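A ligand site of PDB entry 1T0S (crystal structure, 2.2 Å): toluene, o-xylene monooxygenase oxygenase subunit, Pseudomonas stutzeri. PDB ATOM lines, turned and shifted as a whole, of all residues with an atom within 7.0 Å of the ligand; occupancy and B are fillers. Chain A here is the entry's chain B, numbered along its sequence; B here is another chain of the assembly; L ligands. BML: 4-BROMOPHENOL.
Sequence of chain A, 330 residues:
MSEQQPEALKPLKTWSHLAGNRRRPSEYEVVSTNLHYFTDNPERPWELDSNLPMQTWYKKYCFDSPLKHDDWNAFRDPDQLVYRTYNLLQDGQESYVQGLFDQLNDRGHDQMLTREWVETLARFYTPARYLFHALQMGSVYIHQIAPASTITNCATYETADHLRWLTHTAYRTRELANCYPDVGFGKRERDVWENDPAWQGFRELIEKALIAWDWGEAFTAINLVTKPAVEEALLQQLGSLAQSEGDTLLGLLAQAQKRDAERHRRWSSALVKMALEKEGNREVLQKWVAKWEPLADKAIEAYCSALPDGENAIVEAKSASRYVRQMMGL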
ATOM      1  N   GLN A  93      34.061  15.810  10.322  1.00  0.00           N
ATOM      2  CA  GLN A  93      34.664  14.538   9.954  1.00  0.00           C
ATOM      3  C   GLN A  93      33.625  13.526   9.470  1.00  0.00           C
ATOM      4  O   GLN A  93      33.893  12.739   8.556  1.00  0.00           O
ATOM      5  CB  GLN A  93      35.441  13.964  11.141  1.00  0.00           C
ATOM      6  CG  GLN A  93      36.700  14.764  11.488  1.00  0.00           C
ATOM      7  CD  GLN A  93      37.703  14.767  10.347  1.00  0.00           C
ATOM      8  OE1 GLN A  93      38.203  13.711   9.957  1.00  0.00           O
ATOM      9  NE2 GLN A  93      37.997  15.953   9.810  1.00  0.00           N
ATOM     10  N   GLU A  94      32.445  13.553  10.083  1.00  0.00           N
ATOM     11  CA  GLU A  94      31.386  12.635   9.692  1.00  0.00           C
ATOM     12  C   GLU A  94      30.814  13.012   8.329  1.00  0.00           C
ATOM     13  O   GLU A  94      30.321  12.155   7.618  1.00  0.00           O
ATOM     14  CB  GLU A  94      30.260  12.614  10.732  1.00  0.00           C
ATOM     15  CG  GLU A  94      30.559  11.773  11.960  1.00  0.00           C
ATOM     16  CD  GLU A  94      30.841  10.311  11.644  1.00  0.00           C
ATOM     17  OE1 GLU A  94      31.986   9.983  11.243  1.00  0.00           O
ATOM     18  OE2 GLU A  94      29.908   9.489  11.815  1.00  0.00           O
ATOM     19  N   SER A  95      30.867  14.299   7.980  1.00  0.00           N
ATOM     20  CA  SER A  95      30.375  14.725   6.673  1.00  0.00           C
ATOM     21  C   SER A  95      31.298  14.111   5.634  1.00  0.00           C
ATOM     22  O   SER A  95      30.864  13.674   4.580  1.00  0.00           O
ATOM     23  CB  SER A  95      30.408  16.256   6.537  1.00  0.00           C
ATOM     24  OG  SER A  95      29.401  16.870   7.301  1.00  0.00           O
ATOM     25  N   TYR A  96      32.595  14.098   5.966  1.00  0.00           N
ATOM     26  CA  TYR A  96      33.612  13.525   5.091  1.00  0.00           C
ATOM     27  C   TYR A  96      33.375  12.013   4.940  1.00  0.00           C
ATOM     28  O   TYR A  96      33.369  11.478   3.836  1.00  0.00           O
ATOM     29  CB  TYR A  96      35.008  13.801   5.657  1.00  0.00           C
ATOM     30  CG  TYR A  96      36.120  12.993   5.015  1.00  0.00           C
ATOM     31  CD1 TYR A  96      36.412  13.097   3.643  1.00  0.00           C
ATOM     32  CD2 TYR A  96      36.902  12.112   5.780  1.00  0.00           C
ATOM     33  CE1 TYR A  96      37.447  12.353   3.057  1.00  0.00           C
ATOM     34  CE2 TYR A  96      37.939  11.367   5.204  1.00  0.00           C
ATOM     35  CZ  TYR A  96      38.204  11.489   3.843  1.00  0.00           C
ATOM     36  OH  TYR A  96      39.213  10.733   3.288  1.00  0.00           O
ATOM     37  N   VAL A  97      33.174  11.324   6.054  1.00  0.00           N
ATOM     38  CA  VAL A  97      32.951   9.896   5.993  1.00  0.00           C
ATOM     39  C   VAL A  97      31.680   9.580   5.228  1.00  0.00           C
ATOM     40  O   VAL A  97      31.607   8.576   4.507  1.00  0.00           O
ATOM     41  CB  VAL A  97      32.873   9.288   7.419  1.00  0.00           C
ATOM     42  CG1 VAL A  97      32.287   7.859   7.364  1.00  0.00           C
ATOM     43  CG2 VAL A  97      34.279   9.258   8.034  1.00  0.00           C
ATOM     44  N   GLN A  98      30.674  10.427   5.391  1.00  0.00           N
ATOM     45  CA  GLN A  98      29.416  10.209   4.695  1.00  0.00           C
ATOM     46  C   GLN A  98      29.691  10.293   3.203  1.00  0.00           C
ATOM     47  O   GLN A  98      29.163   9.503   2.414  1.00  0.00           O
ATOM     48  CB  GLN A  98      28.367  11.238   5.113  1.00  0.00           C
ATOM     49  CG  GLN A  98      27.077  11.115   4.339  1.00  0.00           C
ATOM     50  CD  GLN A  98      25.973  12.015   4.861  1.00  0.00           C
ATOM     51  OE1 GLN A  98      24.980  12.262   4.179  1.00  0.00           O
ATOM     52  NE2 GLN A  98      26.126  12.493   6.105  1.00  0.00           N
ATOM     53  N   GLY A  99      30.543  11.243   2.817  1.00  0.00           N
ATOM     54  CA  GLY A  99      30.893  11.385   1.420  1.00  0.00           C
ATOM     55  C   GLY A  99      31.497  10.098   0.882  1.00  0.00           C
ATOM     56  O   GLY A  99      31.050   9.584  -0.142  1.00  0.00           O
ATOM     57  N   PHE A 101      31.384   6.901   1.919  1.00  0.00           N
ATOM     58  CA  PHE A 101      30.406   5.813   1.801  1.00  0.00           C
ATOM     59  C   PHE A 101      29.425   6.009   0.637  1.00  0.00           C
ATOM     60  O   PHE A 101      29.299   5.166  -0.240  1.00  0.00           O
ATOM     61  CB  PHE A 101      29.587   5.694   3.090  1.00  0.00           C
ATOM     62  CG  PHE A 101      30.329   5.080   4.239  1.00  0.00           C
ATOM     63  CD1 PHE A 101      29.993   5.384   5.547  1.00  0.00           C
ATOM     64  CD2 PHE A 101      31.367   4.173   4.013  1.00  0.00           C
ATOM     65  CE1 PHE A 101      30.653   4.799   6.621  1.00  0.00           C
ATOM     66  CE2 PHE A 101      32.028   3.588   5.088  1.00  0.00           C
ATOM     67  CZ  PHE A 101      31.671   3.901   6.387  1.00  0.00           C
ATOM     68  N   ASP A 102      28.735   7.139   0.659  1.00  0.00           N
ATOM     69  CA  ASP A 102      27.734   7.464  -0.343  1.00  0.00           C
ATOM     70  C   ASP A 102      28.262   7.533  -1.762  1.00  0.00           C
ATOM     71  O   ASP A 102      27.678   6.925  -2.677  1.00  0.00           O
ATOM     72  CB  ASP A 102      27.067   8.784   0.060  1.00  0.00           C
ATOM     73  CG  ASP A 102      26.039   9.269  -0.949  1.00  0.00           C
ATOM     74  OD1 ASP A 102      25.172   8.461  -1.374  1.00  0.00           O
ATOM     75  OD2 ASP A 102      26.091  10.463  -1.289  1.00  0.00           O
ATOM     76  N   ARG A 164      31.935   5.663  17.643  1.00  0.00           N
ATOM     77  CA  ARG A 164      31.962   6.083  16.250  1.00  0.00           C
ATOM     78  C   ARG A 164      32.642   5.009  15.386  1.00  0.00           C
ATOM     79  O   ARG A 164      32.195   4.708  14.283  1.00  0.00           O
ATOM     80  CB  ARG A 164      32.727   7.411  16.142  1.00  0.00           C
ATOM     81  CG  ARG A 164      32.765   8.008  14.759  1.00  0.00           C
ATOM     82  CD  ARG A 164      33.910   9.016  14.614  1.00  0.00           C
ATOM     83  NE  ARG A 164      33.911   9.566  13.273  1.00  0.00           N
ATOM     84  CZ  ARG A 164      34.979  10.048  12.640  1.00  0.00           C
ATOM     85  NH1 ARG A 164      34.833  10.535  11.419  1.00  0.00           N
ATOM     86  NH2 ARG A 164      36.180  10.044  13.218  1.00  0.00           N
ATOM     87  N   THR A 167      30.310   2.194  15.014  1.00  0.00           N
ATOM     88  CA  THR A 167      29.277   2.579  14.075  1.00  0.00           C
ATOM     89  C   THR A 167      29.722   2.478  12.620  1.00  0.00           C
ATOM     90  O   THR A 167      28.978   1.927  11.777  1.00  0.00           O
ATOM     91  CB  THR A 167      28.785   3.997  14.405  1.00  0.00           C
ATOM     92  OG1 THR A 167      28.393   4.029  15.796  1.00  0.00           O
ATOM     93  CG2 THR A 167      27.572   4.385  13.539  1.00  0.00           C
ATOM     94  N   HIS A 168      30.914   2.977  12.309  1.00  0.00           N
ATOM     95  CA  HIS A 168      31.408   2.885  10.942  1.00  0.00           C
ATOM     96  C   HIS A 168      31.427   1.419  10.523  1.00  0.00           C
ATOM     97  O   HIS A 168      30.983   1.053   9.429  1.00  0.00           O
ATOM     98  CB  HIS A 168      32.837   3.412  10.815  1.00  0.00           C
ATOM     99  CG  HIS A 168      32.992   4.875  11.071  1.00  0.00           C
ATOM    100  ND1 HIS A 168      32.023   5.796  10.751  1.00  0.00           N
ATOM    101  CD2 HIS A 168      34.063   5.593  11.491  1.00  0.00           C
ATOM    102  CE1 HIS A 168      32.479   7.018  10.955  1.00  0.00           C
ATOM    103  NE2 HIS A 168      33.719   6.924  11.401  1.00  0.00           N
ATOM    104  N   TYR A 171      27.917  -0.208   9.836  1.00  0.00           N
ATOM    105  CA  TYR A 171      27.389   0.265   8.562  1.00  0.00           C
ATOM    106  C   TYR A 171      28.087  -0.477   7.418  1.00  0.00           C
ATOM    107  O   TYR A 171      27.437  -1.079   6.558  1.00  0.00           O
ATOM    108  CB  TYR A 171      27.642   1.768   8.441  1.00  0.00           C
ATOM    109  CG  TYR A 171      27.027   2.412   7.223  1.00  0.00           C
ATOM    110  CD1 TYR A 171      25.688   2.800   7.217  1.00  0.00           C
ATOM    111  CD2 TYR A 171      27.781   2.602   6.049  1.00  0.00           C
ATOM    112  CE1 TYR A 171      25.100   3.356   6.097  1.00  0.00           C
ATOM    113  CE2 TYR A 171      27.207   3.171   4.908  1.00  0.00           C
ATOM    114  CZ  TYR A 171      25.856   3.546   4.943  1.00  0.00           C
ATOM    115  OH  TYR A 171      25.255   4.104   3.844  1.00  0.00           O
ATOM    116  N   ARG A 172      29.415  -0.431   7.406  1.00  0.00           N
ATOM    117  CA  ARG A 172      30.154  -1.106   6.350  1.00  0.00           C
ATOM    118  C   ARG A 172      29.831  -2.603   6.286  1.00  0.00           C
ATOM    119  O   ARG A 172      29.739  -3.172   5.207  1.00  0.00           O
ATOM    120  CB  ARG A 172      31.653  -0.904   6.548  1.00  0.00           C
ATOM    121  CG  ARG A 172      32.482  -1.474   5.416  1.00  0.00           C
ATOM    122  CD  ARG A 172      32.105  -0.810   4.111  1.00  0.00           C
ATOM    123  NE  ARG A 172      32.850  -1.372   2.995  1.00  0.00           N
ATOM    124  CZ  ARG A 172      32.447  -1.316   1.730  1.00  0.00           C
ATOM    125  NH1 ARG A 172      33.184  -1.855   0.765  1.00  0.00           N
ATOM    126  NH2 ARG A 172      31.286  -0.725   1.442  1.00  0.00           N
ATOM    127  N   GLU A 175      26.687  -3.173   4.315  1.00  0.00           N
ATOM    128  CA  GLU A 175      26.925  -2.992   2.896  1.00  0.00           C
ATOM    129  C   GLU A 175      27.603  -4.214   2.303  1.00  0.00           C
ATOM    130  O   GLU A 175      27.272  -4.641   1.191  1.00  0.00           O
ATOM    131  CB  GLU A 175      27.771  -1.744   2.623  1.00  0.00           C
ATOM    132  CG  GLU A 175      26.990  -0.442   2.652  1.00  0.00           C
ATOM    133  CD  GLU A 175      27.789   0.746   2.101  1.00  0.00           C
ATOM    134  OE1 GLU A 175      27.146   1.664   1.548  1.00  0.00           O
ATOM    135  OE2 GLU A 175      29.039   0.772   2.225  1.00  0.00           O
ATOM    136  N   SER B   2      24.892   6.140  -3.099  1.00  0.00           N
ATOM    137  CA  SER B   2      23.679   6.006  -2.234  1.00  0.00           C
ATOM    138  C   SER B   2      24.056   5.555  -0.818  1.00  0.00           C
ATOM    139  O   SER B   2      25.197   5.158  -0.558  1.00  0.00           O
ATOM    140  CB  SER B   2      22.703   5.002  -2.842  1.00  0.00           C
ATOM    141  OG  SER B   2      22.355   5.380  -4.160  1.00  0.00           O
ATOM    142  N   MET B   3      23.080   5.627   0.092  1.00  0.00           N
ATOM    143  CA  MET B   3      23.249   5.252   1.502  1.00  0.00           C
ATOM    144  C   MET B   3      22.142   4.319   1.975  1.00  0.00           C
ATOM    145  O   MET B   3      21.033   4.294   1.420  1.00  0.00           O
ATOM    146  CB  MET B   3      23.272   6.516   2.388  1.00  0.00           C
ATOM    147  CG  MET B   3      24.520   7.429   2.205  1.00  0.00           C
ATOM    148  SD  MET B   3      24.395   9.040   3.063  1.00  0.00           S
ATOM    149  CE  MET B   3      23.226   9.808   2.104  1.00  0.00           C
ATOM    150  N   LEU B   4      22.446   3.533   3.003  1.00  0.00           N
ATOM    151  CA  LEU B   4      21.501   2.586   3.586  1.00  0.00           C
ATOM    152  C   LEU B   4      20.467   3.316   4.422  1.00  0.00           C
ATOM    153  O   LEU B   4      20.681   4.455   4.843  1.00  0.00           O
ATOM    154  CB  LEU B   4      22.248   1.602   4.492  1.00  0.00           C
ATOM    155  CG  LEU B   4      23.324   0.698   3.883  1.00  0.00           C
ATOM    156  CD1 LEU B   4      24.151   0.041   4.996  1.00  0.00           C
ATOM    157  CD2 LEU B   4      22.660  -0.343   3.002  1.00  0.00           C
ATOM    158  N   TRP B   9      20.770  -1.275   9.223  1.00  0.00           N
ATOM    159  CA  TRP B   9      22.029  -1.547   9.887  1.00  0.00           C
ATOM    160  C   TRP B   9      22.089  -1.173  11.368  1.00  0.00           C
ATOM    161  O   TRP B   9      23.124  -1.318  12.007  1.00  0.00           O
ATOM    162  CB  TRP B   9      23.155  -0.830   9.141  1.00  0.00           C
ATOM    163  CG  TRP B   9      23.024   0.659   9.146  1.00  0.00           C
ATOM    164  CD1 TRP B   9      22.195   1.424   8.375  1.00  0.00           C
ATOM    165  CD2 TRP B   9      23.751   1.573   9.972  1.00  0.00           C
ATOM    166  NE1 TRP B   9      22.368   2.758   8.659  1.00  0.00           N
ATOM    167  CE2 TRP B   9      23.322   2.877   9.626  1.00  0.00           C
ATOM    168  CE3 TRP B   9      24.737   1.419  10.955  1.00  0.00           C
ATOM    169  CZ2 TRP B   9      23.836   4.030  10.247  1.00  0.00           C
ATOM    170  CZ3 TRP B   9      25.251   2.573  11.566  1.00  0.00           C
ATOM    171  CH2 TRP B   9      24.804   3.850  11.202  1.00  0.00           C
ATOM    172  N   THR B  54      21.857   7.139  15.900  1.00  0.00           N
ATOM    173  CA  THR B  54      23.220   6.699  15.624  1.00  0.00           C
ATOM    174  C   THR B  54      24.184   7.880  15.712  1.00  0.00           C
ATOM    175  O   THR B  54      23.780   9.047  15.605  1.00  0.00           O
ATOM    176  CB  THR B  54      23.353   6.037  14.228  1.00  0.00           C
ATOM    177  OG1 THR B  54      23.185   7.038  13.222  1.00  0.00           O
ATOM    178  CG2 THR B  54      22.297   4.942  14.026  1.00  0.00           C
ATOM    179  N   TYR B  55      25.469   7.569  15.873  1.00  0.00           N
ATOM    180  CA  TYR B  55      26.501   8.595  16.026  1.00  0.00           C
ATOM    181  C   TYR B  55      26.445   9.777  15.063  1.00  0.00           C
ATOM    182  O   TYR B  55      26.348  10.930  15.496  1.00  0.00           O
ATOM    183  CB  TYR B  55      27.883   7.962  15.978  1.00  0.00           C
ATOM    184  CG  TYR B  55      29.002   8.923  16.236  1.00  0.00           C
ATOM    185  CD1 TYR B  55      29.506   9.740  15.212  1.00  0.00           C
ATOM    186  CD2 TYR B  55      29.557   9.045  17.501  1.00  0.00           C
ATOM    187  CE1 TYR B  55      30.540  10.646  15.455  1.00  0.00           C
ATOM    188  CE2 TYR B  55      30.607   9.963  17.753  1.00  0.00           C
ATOM    189  CZ  TYR B  55      31.086  10.747  16.721  1.00  0.00           C
ATOM    190  OH  TYR B  55      32.116  11.610  16.964  1.00  0.00           O
ATOM    191  N   PRO B  56      26.499   9.513  13.745  1.00  0.00           N
ATOM    192  CA  PRO B  56      26.455  10.652  12.811  1.00  0.00           C
ATOM    193  C   PRO B  56      25.228  11.534  13.019  1.00  0.00           C
ATOM    194  O   PRO B  56      25.332  12.767  12.957  1.00  0.00           O
ATOM    195  CB  PRO B  56      26.482   9.979  11.433  1.00  0.00           C
ATOM    196  CG  PRO B  56      25.863   8.659  11.680  1.00  0.00           C
ATOM    197  CD  PRO B  56      26.443   8.239  13.012  1.00  0.00           C
ATOM    198  N   GLU B  57      24.070  10.925  13.257  1.00  0.00           N
ATOM    199  CA  GLU B  57      22.871  11.712  13.484  1.00  0.00           C
ATOM    200  C   GLU B  57      23.038  12.551  14.759  1.00  0.00           C
ATOM    201  O   GLU B  57      22.708  13.733  14.777  1.00  0.00           O
ATOM    202  CB  GLU B  57      21.638  10.812  13.646  1.00  0.00           C
ATOM    203  CG  GLU B  57      21.335   9.921  12.440  1.00  0.00           C
ATOM    204  CD  GLU B  57      20.150   9.003  12.708  1.00  0.00           C
ATOM    205  OE1 GLU B  57      20.142   8.296  13.738  1.00  0.00           O
ATOM    206  OE2 GLU B  57      19.202   8.983  11.892  1.00  0.00           O
HETATM  207  O1  BML L   1      29.275   7.175  10.937  1.00  0.00           O
HETATM  208  C1  BML L   1      28.690   7.141   9.744  1.00  0.00           C
HETATM  209  C2  BML L   1      28.785   8.388   8.921  1.00  0.00           C
HETATM  210  C3  BML L   1      28.131   8.304   7.613  1.00  0.00           C
HETATM  211  C4  BML L   1      27.449   7.131   7.154  1.00  0.00           C
HETATM  212  C5  BML L   1      27.424   6.070   8.023  1.00  0.00           C
HETATM  213  C6  BML L   1      27.947   5.988   9.209  1.00  0.00           C
HETATM  214 BR4  BML L   1      26.673   7.178   5.463  1.00  0.00          BR
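ND1 of His 168 sits at hydrogen-bond distance from O1 of the ligand, at 3.1 Å.
The side-chain carboxylate of Glu 94 sits at hydrogen-bond distance from an oxygen (O1) of the ligand, at 2.6 Å.
Val 97 touches the ligand (CG1 to C2, 3.9 Å).
CA of Gln 98 touches C3 of the ligand (3.7 Å).
Phe 101 touches the ligand.
Tyr 171 touches the ligand (OH to BR4, 3.8 Å).
Met 3 of chain B touches the ligand.
Pro 56 of chain B touches the ligand (CD to O1, 3.7 Å).
Eight residues have an atom within 4 Å of the ligand: Glu 94, Val 97, Gln 98, Phe 101, His 168, Tyr 171, Met 3 of chain B and Pro 56 of chain B.
The nearest printed residue that does not touch the ligand is Thr 167 (4.2 Å).
The side-chain carboxylate of Glu 94 lies within salt-bridge range of the guanidinium group of Arg 164, at 2.8 Å.
The side-chain sulfur (SD) of Met 3 of chain B sits close to the side-chain amide oxygen (OE1) of Gln 98.
The guanidinium group (NE) of Arg 164 lies within hydrogen-bond range of a ring nitrogen (NE2) of His 168 (3.2 Å).
OH of Tyr 171 sits at hydrogen-bond distance from N of Leu 4 of chain B (3.0 Å).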
